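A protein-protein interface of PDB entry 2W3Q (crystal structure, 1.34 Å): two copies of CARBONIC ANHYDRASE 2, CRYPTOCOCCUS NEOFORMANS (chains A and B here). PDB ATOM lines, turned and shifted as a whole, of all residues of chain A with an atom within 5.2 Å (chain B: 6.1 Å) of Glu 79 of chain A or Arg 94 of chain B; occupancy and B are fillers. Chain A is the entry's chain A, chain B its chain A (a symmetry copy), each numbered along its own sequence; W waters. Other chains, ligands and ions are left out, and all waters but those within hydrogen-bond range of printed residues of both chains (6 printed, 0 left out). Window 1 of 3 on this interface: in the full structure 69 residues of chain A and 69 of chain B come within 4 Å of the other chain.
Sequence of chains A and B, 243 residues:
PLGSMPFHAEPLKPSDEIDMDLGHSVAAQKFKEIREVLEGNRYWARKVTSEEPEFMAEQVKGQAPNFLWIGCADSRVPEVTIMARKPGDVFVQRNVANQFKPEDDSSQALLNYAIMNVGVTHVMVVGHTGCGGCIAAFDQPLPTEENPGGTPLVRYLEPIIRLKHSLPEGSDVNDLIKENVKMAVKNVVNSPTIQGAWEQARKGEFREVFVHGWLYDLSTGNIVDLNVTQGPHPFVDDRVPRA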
ATOM      1  N   TRP A  69      15.382  12.581 -20.489  1.00  0.00           N
ATOM      2  CA  TRP A  69      16.538  12.880 -21.325  1.00  0.00           C
ATOM      3  C   TRP A  69      16.359  12.315 -22.725  1.00  0.00           C
ATOM      4  O   TRP A  69      16.231  11.095 -22.858  1.00  0.00           O
ATOM      5  CB  TRP A  69      17.751  12.281 -20.694  1.00  0.00           C
ATOM      6  CG  TRP A  69      19.108  12.324 -21.322  1.00  0.00           C
ATOM      7  CD1 TRP A  69      19.567  11.651 -22.394  1.00  0.00           C
ATOM      8  CD2 TRP A  69      20.213  13.098 -20.845  1.00  0.00           C
ATOM      9  NE1 TRP A  69      20.881  11.973 -22.614  1.00  0.00           N
ATOM     10  CE2 TRP A  69      21.307  12.865 -21.670  1.00  0.00           C
ATOM     11  CE3 TRP A  69      20.386  13.996 -19.765  1.00  0.00           C
ATOM     12  CZ2 TRP A  69      22.566  13.471 -21.487  1.00  0.00           C
ATOM     13  CZ3 TRP A  69      21.604  14.585 -19.586  1.00  0.00           C
ATOM     14  CH2 TRP A  69      22.686  14.329 -20.439  1.00  0.00           C
ATOM     15  N   VAL A  77      28.145   9.504 -24.248  1.00  0.00           N
ATOM     16  CA  VAL A  77      27.179  10.339 -23.537  1.00  0.00           C
ATOM     17  C   VAL A  77      26.169   9.563 -22.702  1.00  0.00           C
ATOM     18  O   VAL A  77      24.954   9.659 -22.875  1.00  0.00           O
ATOM     19  CB  VAL A  77      26.485  11.325 -24.516  1.00  0.00           C
ATOM     20  CG1 VAL A  77      25.809  12.450 -23.778  1.00  0.00           C
ATOM     21  CG2 VAL A  77      27.496  11.939 -25.491  1.00  0.00           C
ATOM     22  N   PRO A  78      26.640   8.780 -21.718  1.00  0.00           N
ATOM     23  CA  PRO A  78      25.755   8.136 -20.743  1.00  0.00           C
ATOM     24  C   PRO A  78      25.250   9.112 -19.685  1.00  0.00           C
ATOM     25  O   PRO A  78      26.018   9.650 -18.904  1.00  0.00           O
ATOM     26  CB  PRO A  78      26.638   7.070 -20.077  1.00  0.00           C
ATOM     27  CG  PRO A  78      28.020   7.651 -20.202  1.00  0.00           C
ATOM     28  CD  PRO A  78      28.044   8.415 -21.461  1.00  0.00           C
ATOM     29  N   GLU A  79      23.955   9.353 -19.691  1.00  0.00           N
ATOM     30  CA  GLU A  79      23.362  10.446 -18.958  1.00  0.00           C
ATOM     31  C   GLU A  79      23.601  10.365 -17.455  1.00  0.00           C
ATOM     32  O   GLU A  79      23.946  11.395 -16.847  1.00  0.00           O
ATOM     33  CB  GLU A  79      21.876  10.518 -19.289  1.00  0.00           C
ATOM     34  CG  GLU A  79      21.035   9.453 -18.633  1.00  0.00           C
ATOM     35  CD  GLU A  79      21.302   8.070 -19.199  1.00  0.00           C
ATOM     36  OE1 GLU A  79      21.578   7.935 -20.405  1.00  0.00           O
ATOM     37  OE2 GLU A  79      21.241   7.107 -18.409  1.00  0.00           O
ATOM     38  N   VAL A  80      23.438   9.188 -16.851  1.00  0.00           N
ATOM     39  CA  VAL A  80      23.544   9.088 -15.388  1.00  0.00           C
ATOM     40  C   VAL A  80      24.959   9.338 -14.917  1.00  0.00           C
ATOM     41  O   VAL A  80      25.225   9.950 -13.906  1.00  0.00           O
ATOM     42  CB  VAL A  80      22.985   7.717 -14.960  1.00  0.00           C
ATOM     43  CG1 VAL A  80      23.404   7.277 -13.574  1.00  0.00           C
ATOM     44  CG2 VAL A  80      21.463   7.808 -15.054  1.00  0.00           C
ATOM     45  N   THR A  81      25.915   8.858 -15.712  1.00  0.00           N
ATOM     46  CA  THR A  81      27.324   9.073 -15.405  1.00  0.00           C
ATOM     47  C   THR A  81      27.723  10.532 -15.468  1.00  0.00           C
ATOM     48  O   THR A  81      28.306  11.065 -14.523  1.00  0.00           O
ATOM     49  CB  THR A  81      28.156   8.240 -16.395  1.00  0.00           C
ATOM     50  OG1 THR A  81      27.912   6.842 -16.196  1.00  0.00           O
ATOM     51  CG2 THR A  81      29.621   8.542 -16.138  1.00  0.00           C
ATOM     52  N   ILE A  82      27.407  11.192 -16.596  1.00  0.00           N
ATOM     53  CA  ILE A  82      27.893  12.561 -16.747  1.00  0.00           C
ATOM     54  C   ILE A  82      27.116  13.566 -15.912  1.00  0.00           C
ATOM     55  O   ILE A  82      27.591  14.673 -15.700  1.00  0.00           O
ATOM     56  CB  ILE A  82      27.905  12.906 -18.232  1.00  0.00           C
ATOM     57  CG1 ILE A  82      26.551  12.896 -18.869  1.00  0.00           C
ATOM     58  CG2 ILE A  82      28.767  11.907 -18.977  1.00  0.00           C
ATOM     59  CD1 ILE A  82      26.592  13.339 -20.318  1.00  0.00           C
ATOM     60  N   MET A  83      25.950  13.257 -15.356  1.00  0.00           N
ATOM     61  CA  MET A  83      25.262  14.109 -14.402  1.00  0.00           C
ATOM     62  C   MET A  83      25.449  13.683 -12.952  1.00  0.00           C
ATOM     63  O   MET A  83      24.875  14.256 -12.026  1.00  0.00           O
ATOM     64  CB  MET A  83      23.768  14.142 -14.757  1.00  0.00           C
ATOM     65  CG  MET A  83      23.572  14.919 -16.064  1.00  0.00           C
ATOM     66  SD  MET A  83      21.856  15.463 -16.118  1.00  0.00           S
ATOM     67  CE  MET A  83      21.112  13.826 -16.126  1.00  0.00           C
ATOM     68  N   ALA A  84      26.234  12.626 -12.738  1.00  0.00           N
ATOM     69  CA  ALA A  84      26.468  12.025 -11.412  1.00  0.00           C
ATOM     70  C   ALA A  84      25.140  11.785 -10.697  1.00  0.00           C
ATOM     71  O   ALA A  84      24.889  12.166  -9.564  1.00  0.00           O
ATOM     72  CB  ALA A  84      27.437  12.875 -10.644  1.00  0.00           C
ATOM     73  N   VAL A  90      16.442   9.548 -13.995  1.00  0.00           N
ATOM     74  CA  VAL A  90      16.326  10.062 -15.373  1.00  0.00           C
ATOM     75  C   VAL A  90      15.718   9.017 -16.282  1.00  0.00           C
ATOM     76  O   VAL A  90      16.310   7.971 -16.487  1.00  0.00           O
ATOM     77  CB  VAL A  90      17.693  10.500 -15.952  1.00  0.00           C
ATOM     78  CG1 VAL A  90      17.457  11.237 -17.273  1.00  0.00           C
ATOM     79  CG2 VAL A  90      18.425  11.426 -14.993  1.00  0.00           C
ATOM     80  N   VAL A  92      14.857   7.856 -20.063  1.00  0.00           N
ATOM     81  CA  VAL A  92      15.736   8.153 -21.209  1.00  0.00           C
ATOM     82  C   VAL A  92      15.254   7.650 -22.540  1.00  0.00           C
ATOM     83  O   VAL A  92      14.860   6.498 -22.700  1.00  0.00           O
ATOM     84  CB  VAL A  92      17.100   7.482 -20.935  1.00  0.00           C
ATOM     85  CG1 VAL A  92      18.031   7.604 -22.121  1.00  0.00           C
ATOM     86  CG2 VAL A  92      17.745   8.092 -19.691  1.00  0.00           C
ATOM     87  N   GLN A  93      15.321   8.490 -23.557  1.00  0.00           N
ATOM     88  CA  GLN A  93      15.298   8.112 -24.945  1.00  0.00           C
ATOM     89  C   GLN A  93      16.667   8.397 -25.567  1.00  0.00           C
ATOM     90  O   GLN A  93      17.155   9.521 -25.418  1.00  0.00           O
ATOM     91  CB  GLN A  93      14.237   8.872 -25.750  1.00  0.00           C
ATOM     92  CG  GLN A  93      14.228   8.416 -27.172  1.00  0.00           C
ATOM     93  CD  GLN A  93      13.369   9.129 -28.178  1.00  0.00           C
ATOM     94  OE1 GLN A  93      12.227   8.809 -28.382  1.00  0.00           O
ATOM     95  NE2 GLN A  93      13.978  10.080 -28.862  1.00  0.00           N
ATOM     96  N   ARG A  94      17.252   7.411 -26.216  1.00  0.00           N
ATOM     97  CA  ARG A  94      18.490   7.653 -26.952  1.00  0.00           C
ATOM     98  C   ARG A  94      18.343   7.075 -28.352  1.00  0.00           C
ATOM     99  O   ARG A  94      17.875   5.917 -28.521  1.00  0.00           O
ATOM    100  CB  ARG A  94      19.734   7.095 -26.232  1.00  0.00           C
ATOM    101  CG  ARG A  94      20.138   8.002 -25.077  1.00  0.00           C
ATOM    102  CD  ARG A  94      21.176   7.368 -24.135  1.00  0.00           C
ATOM    103  NE  ARG A  94      22.494   7.321 -24.770  1.00  0.00           N
ATOM    104  CZ  ARG A  94      23.578   6.770 -24.247  1.00  0.00           C
ATOM    105  NH1 ARG A  94      23.420   6.219 -23.054  1.00  0.00           N
ATOM    106  NH2 ARG A  94      24.755   6.761 -24.864  1.00  0.00           N
ATOM    107  N   LEU A 110       6.641   7.415 -26.317  1.00  0.00           N
ATOM    108  CA  LEU A 110       7.537   7.547 -25.172  1.00  0.00           C
ATOM    109  C   LEU A 110       7.281   8.873 -24.458  1.00  0.00           C
ATOM    110  O   LEU A 110       7.233   8.884 -23.237  1.00  0.00           O
ATOM    111  CB  LEU A 110       8.994   7.421 -25.576  1.00  0.00           C
ATOM    112  CG  LEU A 110      10.047   7.472 -24.483  1.00  0.00           C
ATOM    113  CD1 LEU A 110      11.277   6.637 -24.833  1.00  0.00           C
ATOM    114  CD2 LEU A 110      10.543   8.887 -24.182  1.00  0.00           C
ATOM    115  N   TRP B  69      23.661  -1.609 -26.927  1.00  0.00           N
ATOM    116  CA  TRP B  69      22.625  -1.905 -25.945  1.00  0.00           C
ATOM    117  C   TRP B  69      21.271  -1.388 -26.408  1.00  0.00           C
ATOM    118  O   TRP B  69      21.135  -0.175 -26.597  1.00  0.00           O
ATOM    119  CB  TRP B  69      22.992  -1.255 -24.652  1.00  0.00           C
ATOM    120  CG  TRP B  69      22.115  -1.284 -23.441  1.00  0.00           C
ATOM    121  CD1 TRP B  69      20.957  -0.632 -23.218  1.00  0.00           C
ATOM    122  CD2 TRP B  69      22.387  -2.014 -22.242  1.00  0.00           C
ATOM    123  NE1 TRP B  69      20.495  -0.927 -21.963  1.00  0.00           N
ATOM    124  CE2 TRP B  69      21.361  -1.779 -21.335  1.00  0.00           C
ATOM    125  CE3 TRP B  69      23.436  -2.874 -21.836  1.00  0.00           C
ATOM    126  CZ2 TRP B  69      21.312  -2.346 -20.046  1.00  0.00           C
ATOM    127  CZ3 TRP B  69      23.390  -3.426 -20.588  1.00  0.00           C
ATOM    128  CH2 TRP B  69      22.338  -3.169 -19.700  1.00  0.00           C
ATOM    129  N   ILE B  70      20.311  -2.275 -26.579  1.00  0.00           N
ATOM    130  CA  ILE B  70      18.921  -1.973 -26.931  1.00  0.00           C
ATOM    131  C   ILE B  70      18.133  -2.272 -25.665  1.00  0.00           C
ATOM    132  O   ILE B  70      17.888  -3.419 -25.299  1.00  0.00           O
ATOM    133  CB  ILE B  70      18.430  -2.761 -28.145  1.00  0.00           C
ATOM    134  CG1 ILE B  70      19.285  -2.491 -29.417  1.00  0.00           C
ATOM    135  CG2 ILE B  70      16.941  -2.500 -28.348  1.00  0.00           C
ATOM    136  CD1 ILE B  70      18.930  -3.362 -30.586  1.00  0.00           C
ATOM    137  N   GLY B  71      17.795  -1.178 -24.971  1.00  0.00           N
ATOM    138  CA  GLY B  71      17.217  -1.299 -23.647  1.00  0.00           C
ATOM    139  C   GLY B  71      16.020  -0.427 -23.432  1.00  0.00           C
ATOM    140  O   GLY B  71      15.577   0.286 -24.322  1.00  0.00           O
ATOM    141  N   CYS B  72      15.439  -0.489 -22.248  1.00  0.00           N
ATOM    142  CA  CYS B  72      14.275   0.285 -21.882  1.00  0.00           C
ATOM    143  C   CYS B  72      14.684   1.669 -21.368  1.00  0.00           C
ATOM    144  O   CYS B  72      15.733   1.849 -20.760  1.00  0.00           O
ATOM    145  CB  CYS B  72      13.482  -0.432 -20.796  1.00  0.00           C
ATOM    146  SG  CYS B  72      11.832   0.274 -20.451  1.00  0.00           S
ATOM    147  N   ALA B  73      13.766   2.612 -21.616  1.00  0.00           N
ATOM    148  CA  ALA B  73      13.831   3.970 -21.117  1.00  0.00           C
ATOM    149  C   ALA B  73      13.780   4.083 -19.605  1.00  0.00           C
ATOM    150  O   ALA B  73      14.192   5.140 -19.089  1.00  0.00           O
ATOM    151  CB  ALA B  73      12.652   4.739 -21.724  1.00  0.00           C
ATOM    152  N   ASP B  74      13.282   3.074 -18.926  1.00  0.00           N
ATOM    153  CA  ASP B  74      13.139   3.072 -17.482  1.00  0.00           C
ATOM    154  C   ASP B  74      14.358   3.642 -16.786  1.00  0.00           C
ATOM    155  O   ASP B  74      15.493   3.297 -17.072  1.00  0.00           O
ATOM    156  CB  ASP B  74      12.963   1.613 -17.036  1.00  0.00           C
ATOM    157  CG  ASP B  74      12.449   1.487 -15.628  1.00  0.00           C
ATOM    158  OD1 ASP B  74      13.178   1.777 -14.656  1.00  0.00           O
ATOM    159  OD2 ASP B  74      11.279   1.094 -15.503  1.00  0.00           O
ATOM    160  N   SER B  75      14.099   4.581 -15.885  1.00  0.00           N
ATOM    161  CA  SER B  75      15.145   5.312 -15.207  1.00  0.00           C
ATOM    162  C   SER B  75      16.019   4.421 -14.338  1.00  0.00           C
ATOM    163  O   SER B  75      17.095   4.851 -13.901  1.00  0.00           O
ATOM    164  CB  SER B  75      14.492   6.421 -14.358  1.00  0.00           C
ATOM    165  OG  SER B  75      13.730   5.913 -13.310  1.00  0.00           O
ATOM    166  N   ARG B  76      15.573   3.205 -14.055  1.00  0.00           N
ATOM    167  CA  ARG B  76      16.334   2.346 -13.156  1.00  0.00           C
ATOM    168  C   ARG B  76      17.332   1.489 -13.899  1.00  0.00           C
ATOM    169  O   ARG B  76      18.057   0.704 -13.265  1.00  0.00           O
ATOM    170  CB  ARG B  76      15.421   1.425 -12.335  1.00  0.00           C
ATOM    171  CG  ARG B  76      14.450   2.219 -11.482  1.00  0.00           C
ATOM    172  CD  ARG B  76      13.314   1.371 -10.945  1.00  0.00           C
ATOM    173  NE  ARG B  76      12.420   0.954 -12.028  1.00  0.00           N
ATOM    174  CZ  ARG B  76      11.350   0.171 -11.894  1.00  0.00           C
ATOM    175  NH1 ARG B  76      11.010  -0.339 -10.733  1.00  0.00           N
ATOM    176  NH2 ARG B  76      10.606  -0.138 -12.949  1.00  0.00           N
ATOM    177  N   VAL B  77      17.421   1.673 -15.231  1.00  0.00           N
ATOM    178  CA  VAL B  77      18.328   0.837 -16.014  1.00  0.00           C
ATOM    179  C   VAL B  77      19.322   1.612 -16.868  1.00  0.00           C
ATOM    180  O   VAL B  77      19.391   1.480 -18.090  1.00  0.00           O
ATOM    181  CB  VAL B  77      17.526  -0.197 -16.854  1.00  0.00           C
ATOM    182  CG1 VAL B  77      18.410  -1.314 -17.340  1.00  0.00           C
ATOM    183  CG2 VAL B  77      16.390  -0.815 -16.032  1.00  0.00           C
ATOM    184  N   PRO B  78      20.176   2.437 -16.240  1.00  0.00           N
ATOM    185  CA  PRO B  78      21.287   3.089 -16.939  1.00  0.00           C
ATOM    186  C   PRO B  78      22.447   2.133 -17.201  1.00  0.00           C
ATOM    187  O   PRO B  78      23.078   1.639 -16.280  1.00  0.00           O
ATOM    188  CB  PRO B  78      21.742   4.196 -15.979  1.00  0.00           C
ATOM    189  CG  PRO B  78      21.366   3.647 -14.629  1.00  0.00           C
ATOM    190  CD  PRO B  78      20.146   2.845 -14.825  1.00  0.00           C
ATOM    191  N   GLU B  79      22.699   1.859 -18.465  1.00  0.00           N
ATOM    192  CA  GLU B  79      23.561   0.774 -18.870  1.00  0.00           C
ATOM    193  C   GLU B  79      24.986   0.908 -18.349  1.00  0.00           C
ATOM    194  O   GLU B  79      25.541  -0.093 -17.861  1.00  0.00           O
ATOM    195  CB  GLU B  79      23.526   0.654 -20.390  1.00  0.00           C
ATOM    196  CG  GLU B  79      24.305   1.718 -21.120  1.00  0.00           C
ATOM    197  CD  GLU B  79      23.663   3.089 -21.011  1.00  0.00           C
ATOM    198  OE1 GLU B  79      22.423   3.193 -20.977  1.00  0.00           O
ATOM    199  OE2 GLU B  79      24.426   4.074 -20.948  1.00  0.00           O
ATOM    200  N   VAL B  92      24.060   3.112 -27.505  1.00  0.00           N
ATOM    201  CA  VAL B  92      22.773   2.802 -26.855  1.00  0.00           C
ATOM    202  C   VAL B  92      21.548   3.252 -27.600  1.00  0.00           C
ATOM    203  O   VAL B  92      21.439   4.387 -28.052  1.00  0.00           O
ATOM    204  CB  VAL B  92      22.760   3.516 -25.484  1.00  0.00           C
ATOM    205  CG1 VAL B  92      21.421   3.380 -24.797  1.00  0.00           C
ATOM    206  CG2 VAL B  92      23.871   2.961 -24.593  1.00  0.00           C
ATOM    207  N   GLN B  93      20.560   2.383 -27.705  1.00  0.00           N
ATOM    208  CA  GLN B  93      19.194   2.717 -28.007  1.00  0.00           C
ATOM    209  C   GLN B  93      18.325   2.448 -26.775  1.00  0.00           C
ATOM    210  O   GLN B  93      18.405   1.341 -26.234  1.00  0.00           O
ATOM    211  CB  GLN B  93      18.629   1.905 -29.180  1.00  0.00           C
ATOM    212  CG  GLN B  93      17.225   2.317 -29.477  1.00  0.00           C
ATOM    213  CD  GLN B  93      16.423   1.551 -30.492  1.00  0.00           C
ATOM    214  OE1 GLN B  93      16.436   1.836 -31.661  1.00  0.00           O
ATOM    215  NE2 GLN B  93      15.658   0.596 -29.997  1.00  0.00           N
ATOM    216  N   ARG B  94      17.551   3.428 -26.358  1.00  0.00           N
ATOM    217  CA  ARG B  94      16.595   3.195 -25.278  1.00  0.00           C
ATOM    218  C   ARG B  94      15.235   3.725 -25.711  1.00  0.00           C
ATOM    219  O   ARG B  94      15.131   4.865 -26.238  1.00  0.00           O
ATOM    220  CB  ARG B  94      17.045   3.806 -23.937  1.00  0.00           C
ATOM    221  CG  ARG B  94      18.123   2.945 -23.290  1.00  0.00           C
ATOM    222  CD  ARG B  94      18.829   3.634 -22.110  1.00  0.00           C
ATOM    223  NE  ARG B  94      17.949   3.695 -20.940  1.00  0.00           N
ATOM    224  CZ  ARG B  94      18.239   4.290 -19.794  1.00  0.00           C
ATOM    225  NH1 ARG B  94      19.425   4.873 -19.735  1.00  0.00           N
ATOM    226  NH2 ARG B  94      17.405   4.309 -18.759  1.00  0.00           N
ATOM    227  N   ASN B  95      14.234   2.881 -25.495  1.00  0.00           N
ATOM    228  CA  ASN B  95      12.853   3.205 -25.851  1.00  0.00           C
ATOM    229  C   ASN B  95      11.942   2.486 -24.868  1.00  0.00           C
ATOM    230  O   ASN B  95      12.440   1.770 -23.991  1.00  0.00           O
ATOM    231  CB  ASN B  95      12.505   2.881 -27.312  1.00  0.00           C
ATOM    232  CG  ASN B  95      12.618   1.412 -27.646  1.00  0.00           C
ATOM    233  OD1 ASN B  95      12.429   0.539 -26.811  1.00  0.00           O
ATOM    234  ND2 ASN B  95      12.963   1.108 -28.886  1.00  0.00           N
ATOM    235  N   VAL B  96      10.623   2.634 -24.999  1.00  0.00           N
ATOM    236  CA  VAL B  96       9.741   2.021 -24.016  1.00  0.00           C
ATOM    237  C   VAL B  96       9.680   0.516 -24.265  1.00  0.00           C
ATOM    238  O   VAL B  96       9.350   0.014 -25.335  1.00  0.00           O
ATOM    239  CB  VAL B  96       8.344   2.659 -24.050  1.00  0.00           C
ATOM    240  CG1 VAL B  96       7.377   1.847 -23.176  1.00  0.00           C
ATOM    241  CG2 VAL B  96       8.447   4.124 -23.651  1.00  0.00           C
HETATM  242  O   HOH W   1      21.423   5.547 -21.394  1.00  0.00           O
HETATM  243  O   HOH W   2      26.485   4.874 -23.109  1.00  0.00           O
HETATM  244  O   HOH W   3      15.036   5.345 -29.165  1.00  0.00           O
HETATM  245  O   HOH W   4      18.459   7.434 -13.850  1.00  0.00           O
HETATM  246  O   HOH W   5      18.742   6.293 -16.781  1.00  0.00           O
HETATM  247  O   HOH W   6      23.712   5.619 -18.609  1.00  0.00           O
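The backbone NH of Val 92 of chain A is in hydrogen-bond range of the backbone carbonyl oxygen of Ala 73 of chain B (3.0 Å). The side-chain carboxylate (OE2) of Glu 79 of chain A lies within salt-bridge range of the guanidinium group (NH1) of Arg 94 of chain B (3.2 Å). The backbone NH (N) of Arg 94 of chain A sits at hydrogen-bond distance from the backbone carbonyl oxygen (O) of Arg 94 of chain B, at 3.3 Å. NH1 of Arg 94 of chain A lies within salt-bridge range of OE2 of Glu 79 of chain B (3.2 Å).
Among the printed residues, merely in contact across the chains: Val 90 of chain A with Ser 75 of chain B (3.2 Å), Gln 93 of chain A with Arg 94 of chain B (3.5 Å), Arg 94 of chain A with Gln 93 of chain B (3.5 Å), Arg 94 of chain A with Val 92 of chain B (3.6 Å), Val 92 of chain A with Arg 94 of chain B (3.6 Å), Val 80 of chain A with Pro 78 of chain B (3.7 Å), Leu 110 of chain A with Val 96 of chain B (3.8 Å), Pro 78 of chain A with Glu 79 of chain B (3.8 Å), Glu 79 of chain A with Pro 78 of chain B (3.8 Å), Leu 110 of chain A with Ala 73 of chain B (3.9 Å) and Leu 110 of chain A with Asn 95 of chain B (3.9 Å).
The side-chain carboxylate of Glu 79 of chain A is in salt-bridge range of the guanidinium group of Arg 94 of chain A. The side-chain amide nitrogen of Asn 95 of chain B sits close to the side-chain amide nitrogen of Gln 93 of chain B (3.0 Å). The backbone carbonyl oxygen (O) of Asn 95 of chain B sits at hydrogen-bond distance from the backbone NH (N) of Ala 73 of chain B, at 2.8 Å. The backbone NH (N) of Gln 93 of chain A lies within hydrogen-bond range of the backbone carbonyl oxygen (O) of Trp 69 of chain A, at 2.8 Å. The guanidinium group (NH1) of Arg 94 of chain B is in salt-bridge range of the side-chain carboxylate (OE1) of Glu 79 of chain B (3.7 Å). NE of Arg 94 of chain B is in hydrogen-bond range of O of Cys 72 of chain B (2.9 Å).
Glu 79 of chain A touches just these residues of chain B: Pro 78 (3.8 Å) and Arg 94 (3.2 Å). Printed residues of chain A within 4 Å of Val 92 of chain B: Arg 94. Of the printed residues of chain B, Pro 78 of chain A touches Glu 79 (3.8 Å). Val 77 of chain A touches none of the printed residues of chain B. Trp 69 of chain A touches none of the printed residues of chain B. The nearest residue of chain B that does not touch Glu 79 of chain A is Glu 79 of chain B (4.8 Å). The nearest printed residue of chain A that does not touch Arg 94 of chain B is Val 90 of chain A (4.4 Å).
Glu 79 of chain A touches Arg 94 of chain B, and with the chains exchanged Arg 94 of chain A touches Glu 79 of chain B. Val 92 of chain A touches Arg 94 of chain B, and with the chains exchanged Arg 94 of chain A touches Val 92 of chain B. Gln 93 of chain A touches Arg 94 of chain B, and with the chains exchanged Arg 94 of chain A touches Gln 93 of chain B. Arg 94 of chain B touches its own counterpart, Arg 94 of chain A. Positions printed for both chains: 69, 77, 78, 79, 92, 93 and 94. Of the 15 pairs that touch across the chains among the printed residues, 9 have their exchanged pair printed and touching as well.
Of the 16 printed residues of chain B, 9 touch a printed residue of chain A. Hydrophobic or aromatic side chains of chain A that line the printed part of chain B: Pro 78, Val 80, Val 92 and Leu 110. Among the printed residues, 15 pairs touch across the chains.
Water W1 lies within hydrogen-bond range of OE1 of Glu 79 of chain A (2.6 Å), OE1 of Glu 79 of chain B (2.6 Å), NH1 of Arg 94 of chain A (2.7 Å) and NH1 of Arg 94 of chain B (2.7 Å). Water W6 bridges the side-chain carboxylate (OE2) of Glu 79 of chain A and the side-chain carboxylate (OE2) of Glu 79 of chain B. Water W4 bridges the backbone carbonyl oxygen (O) of Ser 75 of chain B (2.9 Å) and the backbone NH (N) of Val 90 of chain A (2.9 Å). Water W3 lies within hydrogen-bond range of O of Arg 94 of chain A (3.0 Å) and O of Arg 94 of chain B (3.0 Å). Water W5 lies within hydrogen-bond range of the backbone carbonyl oxygen (O) of Val 90 of chain A, the side-chain carboxylate (OE2) of Glu 79 of chain A and the guanidinium group (NH2) of Arg 94 of chain B. Water W2 bridges OE2 of Glu 79 of chain B (3.1 Å) and NH2 of Arg 94 of chain A (3.1 Å).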
